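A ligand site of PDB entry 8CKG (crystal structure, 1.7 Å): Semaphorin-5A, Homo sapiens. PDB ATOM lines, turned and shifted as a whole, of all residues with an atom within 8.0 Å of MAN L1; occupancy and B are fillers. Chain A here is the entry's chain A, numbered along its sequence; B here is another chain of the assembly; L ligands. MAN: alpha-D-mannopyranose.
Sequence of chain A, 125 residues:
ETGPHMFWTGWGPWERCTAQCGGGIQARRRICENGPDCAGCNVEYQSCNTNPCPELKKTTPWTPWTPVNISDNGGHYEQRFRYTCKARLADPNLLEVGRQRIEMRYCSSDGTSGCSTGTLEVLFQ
The backbone carbonyl oxygen (O) of Cys 41 is in hydrogen-bond range of the guanidinium group (NE) of Arg 30 (3.0 Å).
The backbone carbonyl oxygen (O) of Phe 7 lies within hydrogen-bond range of the backbone NH (N) of Glu 33.
The side-chain sulfur (SG) of Cys 38 of chain A is disulfide-bonded to the side-chain sulfur (SG) of Cys 32, at 2.0 Å.
The indole nitrogen (NE1) of Trp 8 lies within hydrogen-bond range of the backbone carbonyl oxygen (O) of Ala 39.
N of Arg 30 is in hydrogen-bond range of O of Asn 42 (3.0 Å).
SG of Cys 38 of chain A lies within hydrogen-bond range of N of Phe 7 (3.5 Å).
The side-chain sulfur of Cys 38 of chain A lies within hydrogen-bond range of the backbone NH of Trp 8, at 3.7 Å.
The backbone NH (N) of Trp 8 lies close to an oxygen (O2) of MAN L1 (3.1 Å).
An oxygen (O6) of MAN L1 lies within hydrogen-bond range of the guanidinium group (NH1) of Arg 30, at 3.0 Å.
O2 of MAN L2 sits at hydrogen-bond distance from N of Trp 11 (2.7 Å).
CD1 of Trp 11 is bonded to C1 of MAN L2.
A carbon (C1) of MAN L1 is bonded to the aromatic ring (CD1) of Trp 8 (1.5 Å).
O4 of MAN L1 sits at hydrogen-bond distance from O of Ala 39 (2.9 Å).
Residues that only touch MAN L1: Phe 7.
Hydrophobic or aromatic side chains within 4 Å of MAN L1: Trp 8 and Ala 39.
Within 4 Å of MAN L1: Phe 7, Trp 8, Arg 30 and Ala 39.
Along chain A the residues within 4 Å of MAN L1 span positions 7 to 39.
The nearest printed residue that does not touch MAN L1 is Cys 38 of chain A (4.1 Å).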
ATOM      1  N   MET A   6     -34.671   8.631 -21.962  1.00  0.00           N
ATOM      2  CA  MET A   6     -33.300   8.368 -21.517  1.00  0.00           C
ATOM      3  C   MET A   6     -33.229   7.332 -20.406  1.00  0.00           C
ATOM      4  O   MET A   6     -33.744   7.565 -19.308  1.00  0.00           O
ATOM      5  CB  MET A   6     -32.636   9.650 -21.039  1.00  0.00           C
ATOM      6  CG  MET A   6     -32.627  10.787 -22.024  1.00  0.00           C
ATOM      7  SD  MET A   6     -31.593  12.092 -21.348  1.00  0.00           S
ATOM      8  CE  MET A   6     -32.045  13.453 -22.413  1.00  0.00           C
ATOM      9  N   PHE A   7     -32.567   6.211 -20.670  1.00  0.00           N
ATOM     10  CA  PHE A   7     -32.385   5.159 -19.687  1.00  0.00           C
ATOM     11  C   PHE A   7     -30.998   4.552 -19.864  1.00  0.00           C
ATOM     12  O   PHE A   7     -30.526   4.403 -21.001  1.00  0.00           O
ATOM     13  CB  PHE A   7     -33.469   4.080 -19.803  1.00  0.00           C
ATOM     14  CG  PHE A   7     -33.601   3.536 -21.197  1.00  0.00           C
ATOM     15  CD1 PHE A   7     -34.446   4.139 -22.120  1.00  0.00           C
ATOM     16  CD2 PHE A   7     -32.882   2.419 -21.596  1.00  0.00           C
ATOM     17  CE1 PHE A   7     -34.567   3.644 -23.401  1.00  0.00           C
ATOM     18  CE2 PHE A   7     -32.991   1.917 -22.875  1.00  0.00           C
ATOM     19  CZ  PHE A   7     -33.838   2.532 -23.792  1.00  0.00           C
ATOM     20  N   TRP A   8     -30.362   4.194 -18.760  1.00  0.00           N
ATOM     21  CA  TRP A   8     -29.073   3.503 -18.845  1.00  0.00           C
ATOM     22  C   TRP A   8     -29.260   2.106 -19.412  1.00  0.00           C
ATOM     23  O   TRP A   8     -30.285   1.461 -19.209  1.00  0.00           O
ATOM     24  CB  TRP A   8     -28.417   3.383 -17.474  1.00  0.00           C
ATOM     25  CG  TRP A   8     -28.053   4.662 -16.792  1.00  0.00           C
ATOM     26  CD1 TRP A   8     -28.684   5.229 -15.714  1.00  0.00           C
ATOM     27  CD2 TRP A   8     -26.941   5.525 -17.102  1.00  0.00           C
ATOM     28  NE1 TRP A   8     -28.046   6.390 -15.353  1.00  0.00           N
ATOM     29  CE2 TRP A   8     -26.979   6.594 -16.182  1.00  0.00           C
ATOM     30  CE3 TRP A   8     -25.940   5.505 -18.077  1.00  0.00           C
ATOM     31  CZ2 TRP A   8     -26.042   7.646 -16.219  1.00  0.00           C
ATOM     32  CZ3 TRP A   8     -24.998   6.542 -18.099  1.00  0.00           C
ATOM     33  CH2 TRP A   8     -25.070   7.597 -17.175  1.00  0.00           C
ATOM     34  N   THR A   9     -28.235   1.639 -20.115  1.00  0.00           N
ATOM     35  CA  THR A   9     -28.145   0.201 -20.351  1.00  0.00           C
ATOM     36  C   THR A   9     -27.587  -0.472 -19.096  1.00  0.00           C
ATOM     37  O   THR A   9     -27.122   0.188 -18.159  1.00  0.00           O
ATOM     38  CB  THR A   9     -27.259  -0.094 -21.561  1.00  0.00           C
ATOM     39  OG1 THR A   9     -25.882  -0.036 -21.169  1.00  0.00           O
ATOM     40  CG2 THR A   9     -27.505   0.893 -22.692  1.00  0.00           C
ATOM     41  N   GLY A  10     -27.637  -1.798 -19.085  1.00  0.00           N
ATOM     42  CA  GLY A  10     -26.986  -2.522 -18.023  1.00  0.00           C
ATOM     43  C   GLY A  10     -25.488  -2.283 -18.026  1.00  0.00           C
ATOM     44  O   GLY A  10     -24.902  -1.922 -19.048  1.00  0.00           O
ATOM     45  N   TRP A  11     -24.868  -2.470 -16.870  1.00  0.00           N
ATOM     46  CA  TRP A  11     -23.425  -2.294 -16.763  1.00  0.00           C
ATOM     47  C   TRP A  11     -22.698  -3.292 -17.647  1.00  0.00           C
ATOM     48  O   TRP A  11     -23.066  -4.476 -17.713  1.00  0.00           O
ATOM     49  CB  TRP A  11     -22.968  -2.450 -15.316  1.00  0.00           C
ATOM     50  CG  TRP A  11     -23.309  -1.309 -14.411  1.00  0.00           C
ATOM     51  CD1 TRP A  11     -24.290  -1.276 -13.455  1.00  0.00           C
ATOM     52  CD2 TRP A  11     -22.656  -0.035 -14.340  1.00  0.00           C
ATOM     53  NE1 TRP A  11     -24.301  -0.056 -12.819  1.00  0.00           N
ATOM     54  CE2 TRP A  11     -23.302   0.727 -13.340  1.00  0.00           C
ATOM     55  CE3 TRP A  11     -21.593   0.552 -15.042  1.00  0.00           C
ATOM     56  CZ2 TRP A  11     -22.918   2.024 -13.013  1.00  0.00           C
ATOM     57  CZ3 TRP A  11     -21.208   1.837 -14.721  1.00  0.00           C
ATOM     58  CH2 TRP A  11     -21.868   2.561 -13.713  1.00  0.00           C
ATOM     59  N   ARG A  30     -21.431   1.757 -18.789  1.00  0.00           N
ATOM     60  CA  ARG A  30     -22.766   1.644 -19.379  1.00  0.00           C
ATOM     61  C   ARG A  30     -23.074   2.949 -20.107  1.00  0.00           C
ATOM     62  O   ARG A  30     -22.416   3.974 -19.901  1.00  0.00           O
ATOM     63  CB  ARG A  30     -23.825   1.337 -18.307  1.00  0.00           C
ATOM     64  CG  ARG A  30     -24.027   2.478 -17.341  1.00  0.00           C
ATOM     65  CD  ARG A  30     -25.061   2.156 -16.279  1.00  0.00           C
ATOM     66  NE  ARG A  30     -25.207   3.277 -15.369  1.00  0.00           N
ATOM     67  CZ  ARG A  30     -26.030   3.308 -14.329  1.00  0.00           C
ATOM     68  NH1 ARG A  30     -26.791   2.276 -14.034  1.00  0.00           N
ATOM     69  NH2 ARG A  30     -26.079   4.398 -13.569  1.00  0.00           N
ATOM     70  N   ILE A  31     -24.096   2.901 -20.960  1.00  0.00           N
ATOM     71  CA  ILE A  31     -24.391   4.005 -21.875  1.00  0.00           C
ATOM     72  C   ILE A  31     -25.810   4.514 -21.604  1.00  0.00           C
ATOM     73  O   ILE A  31     -26.729   3.726 -21.387  1.00  0.00           O
ATOM     74  CB  ILE A  31     -24.250   3.581 -23.347  1.00  0.00           C
ATOM     75  N   CYS A  32     -25.962   5.830 -21.627  1.00  0.00           N
ATOM     76  CA  CYS A  32     -27.280   6.457 -21.499  1.00  0.00           C
ATOM     77  C   CYS A  32     -27.903   6.558 -22.887  1.00  0.00           C
ATOM     78  O   CYS A  32     -27.536   7.412 -23.687  1.00  0.00           O
ATOM     79  CB  CYS A  32     -27.177   7.831 -20.850  1.00  0.00           C
ATOM     80  SG  CYS A  32     -28.751   8.712 -20.770  1.00  0.00           S
ATOM     81  N   GLU A  33     -28.869   5.691 -23.171  1.00  0.00           N
ATOM     82  CA  GLU A  33     -29.516   5.676 -24.476  1.00  0.00           C
ATOM     83  C   GLU A  33     -30.538   6.795 -24.595  1.00  0.00           C
ATOM     84  O   GLU A  33     -31.207   7.142 -23.617  1.00  0.00           O
ATOM     85  CB  GLU A  33     -30.178   4.319 -24.736  1.00  0.00           C
ATOM     86  CG  GLU A  33     -29.187   3.203 -25.021  1.00  0.00           C
ATOM     87  CD  GLU A  33     -29.853   1.946 -25.552  1.00  0.00           C
ATOM     88  OE1 GLU A  33     -31.052   1.736 -25.254  1.00  0.00           O
ATOM     89  OE2 GLU A  33     -29.194   1.172 -26.279  1.00  0.00           O
ATOM     90  N   ASP A  37     -28.377  12.853 -20.520  1.00  0.00           N
ATOM     91  CA  ASP A  37     -28.576  13.219 -19.110  1.00  0.00           C
ATOM     92  C   ASP A  37     -29.356  12.165 -18.324  1.00  0.00           C
ATOM     93  O   ASP A  37     -30.321  12.506 -17.634  1.00  0.00           O
ATOM     94  CB  ASP A  37     -29.270  14.571 -19.035  1.00  0.00           C
ATOM     95  CG  ASP A  37     -28.376  15.714 -19.447  1.00  0.00           C
ATOM     96  OD1 ASP A  37     -27.147  15.498 -19.581  1.00  0.00           O
ATOM     97  OD2 ASP A  37     -28.900  16.833 -19.622  1.00  0.00           O
ATOM     98  N   CYS A  38     -28.959  10.905 -18.386  1.00  0.00           N
ATOM     99  CA  CYS A  38     -29.476   9.960 -17.400  1.00  0.00           C
ATOM    100  C   CYS A  38     -28.940  10.327 -16.022  1.00  0.00           C
ATOM    101  O   CYS A  38     -27.872  10.917 -15.887  1.00  0.00           O
ATOM    102  CB  CYS A  38     -29.067   8.525 -17.751  1.00  0.00           C
ATOM    103  SG  CYS A  38     -29.772   7.819 -19.253  1.00  0.00           S
ATOM    104  N   ALA A  39     -29.704   9.976 -14.995  1.00  0.00           N
ATOM    105  CA  ALA A  39     -29.270  10.252 -13.626  1.00  0.00           C
ATOM    106  C   ALA A  39     -28.281   9.204 -13.158  1.00  0.00           C
ATOM    107  O   ALA A  39     -28.563   8.003 -13.198  1.00  0.00           O
ATOM    108  CB  ALA A  39     -30.468  10.307 -12.686  1.00  0.00           C
ATOM    109  N   GLY A  40     -27.122   9.654 -12.711  1.00  0.00           N
ATOM    110  CA  GLY A  40     -26.111   8.754 -12.199  1.00  0.00           C
ATOM    111  C   GLY A  40     -24.867   8.729 -13.056  1.00  0.00           C
ATOM    112  O   GLY A  40     -24.603   9.633 -13.858  1.00  0.00           O
ATOM    113  N   CYS A  41     -24.113   7.639 -12.917  1.00  0.00           N
ATOM    114  CA  CYS A  41     -22.769   7.537 -13.456  1.00  0.00           C
ATOM    115  C   CYS A  41     -22.699   6.464 -14.536  1.00  0.00           C
ATOM    116  O   CYS A  41     -23.430   5.466 -14.497  1.00  0.00           O
ATOM    117  CB  CYS A  41     -21.776   7.215 -12.330  1.00  0.00           C
ATOM    118  SG  CYS A  41     -21.874   8.368 -10.951  1.00  0.00           S
ATOM    119  N   ASN A  42     -21.816   6.698 -15.498  1.00  0.00           N
ATOM    120  CA  ASN A  42     -21.586   5.752 -16.593  1.00  0.00           C
ATOM    121  C   ASN A  42     -20.366   4.874 -16.369  1.00  0.00           C
ATOM    122  O   ASN A  42     -20.147   3.929 -17.144  1.00  0.00           O
ATOM    123  CB  ASN A  42     -21.428   6.496 -17.929  1.00  0.00           C
ATOM    124  CG  ASN A  42     -20.106   7.256 -18.027  1.00  0.00           C
ATOM    125  OD1 ASN A  42     -19.025   6.672 -18.024  1.00  0.00           O
ATOM    126  ND2 ASN A  42     -20.199   8.574 -18.150  1.00  0.00           N
ATOM    127  N   PRO B  36     -32.233  13.433  -5.094  1.00  0.00           N
ATOM    128  CA  PRO B  36     -31.373  12.252  -5.222  1.00  0.00           C
ATOM    129  C   PRO B  36     -30.794  12.045  -6.613  1.00  0.00           C
ATOM    130  O   PRO B  36     -29.970  11.140  -6.796  1.00  0.00           O
ATOM    131  CB  PRO B  36     -32.346  11.110  -4.884  1.00  0.00           C
ATOM    132  CG  PRO B  36     -33.662  11.598  -5.413  1.00  0.00           C
ATOM    133  CD  PRO B  36     -33.659  13.096  -5.176  1.00  0.00           C
ATOM    134  N   ASP B  37     -31.188  12.850  -7.596  1.00  0.00           N
ATOM    135  CA  ASP B  37     -31.003  12.479  -8.986  1.00  0.00           C
ATOM    136  C   ASP B  37     -30.718  13.708  -9.861  1.00  0.00           C
ATOM    137  O   ASP B  37     -31.446  14.012 -10.802  1.00  0.00           O
ATOM    138  CB  ASP B  37     -32.252  11.735  -9.479  1.00  0.00           C
ATOM    139  CG  ASP B  37     -33.512  12.391  -8.988  1.00  0.00           C
ATOM    140  OD1 ASP B  37     -33.431  13.466  -8.367  1.00  0.00           O
ATOM    141  OD2 ASP B  37     -34.613  11.833  -9.215  1.00  0.00           O
ATOM    142  N   CYS B  38     -29.634  14.425  -9.574  1.00  0.00           N
ATOM    143  CA  CYS B  38     -29.152  15.424 -10.504  1.00  0.00           C
ATOM    144  C   CYS B  38     -28.623  14.735 -11.753  1.00  0.00           C
ATOM    145  O   CYS B  38     -28.195  13.582 -11.717  1.00  0.00           O
ATOM    146  CB  CYS B  38     -28.072  16.276  -9.861  1.00  0.00           C
ATOM    147  SG  CYS B  38     -28.561  17.297  -8.433  1.00  0.00           S
ATOM    148  N   GLY B  40     -26.292  13.430 -14.473  1.00  0.00           N
ATOM    149  CA  GLY B  40     -24.902  13.070 -14.392  1.00  0.00           C
ATOM    150  C   GLY B  40     -24.518  12.495 -13.038  1.00  0.00           C
ATOM    151  O   GLY B  40     -25.339  12.021 -12.247  1.00  0.00           O
HETATM  152  C1  MAN L   1     -29.838   4.637 -14.981  1.00  0.00           C
HETATM  153  C2  MAN L   1     -30.979   5.650 -15.052  1.00  0.00           C
HETATM  154  C3  MAN L   1     -32.018   5.366 -13.972  1.00  0.00           C
HETATM  155  C4  MAN L   1     -31.368   5.250 -12.595  1.00  0.00           C
HETATM  156  C5  MAN L   1     -30.189   4.274 -12.621  1.00  0.00           C
HETATM  157  C6  MAN L   1     -30.582   2.830 -12.862  1.00  0.00           C
HETATM  158  O2  MAN L   1     -31.594   5.582 -16.336  1.00  0.00           O
HETATM  159  O3  MAN L   1     -32.770   4.202 -14.297  1.00  0.00           O
HETATM  160  O4  MAN L   1     -30.895   6.529 -12.170  1.00  0.00           O
HETATM  161  O5  MAN L   1     -29.273   4.641 -13.665  1.00  0.00           O
HETATM  162  O6  MAN L   1     -29.460   1.966 -12.795  1.00  0.00           O
HETATM  163  C1  MAN L   2     -25.152  -2.437 -13.059  1.00  0.00           C
HETATM  164  C2  MAN L   2     -26.569  -2.044 -13.460  1.00  0.00           C
HETATM  165  C3  MAN L   2     -27.585  -2.947 -12.763  1.00  0.00           C
HETATM  166  C4  MAN L   2     -27.346  -2.965 -11.259  1.00  0.00           C
HETATM  167  C5  MAN L   2     -25.884  -3.291 -10.935  1.00  0.00           C
HETATM  168  C6  MAN L   2     -25.476  -4.702 -11.302  1.00  0.00           C
HETATM  169  O2  MAN L   2     -26.724  -2.157 -14.881  1.00  0.00           O
HETATM  170  O3  MAN L   2     -27.583  -4.257 -13.317  1.00  0.00           O
HETATM  171  O4  MAN L   2     -27.642  -1.680 -10.714  1.00  0.00           O
HETATM  172  O5  MAN L   2     -25.019  -2.392 -11.637  1.00  0.00           O
HETATM  173  O6  MAN L   2     -24.073  -4.909 -11.156  1.00  0.00           O
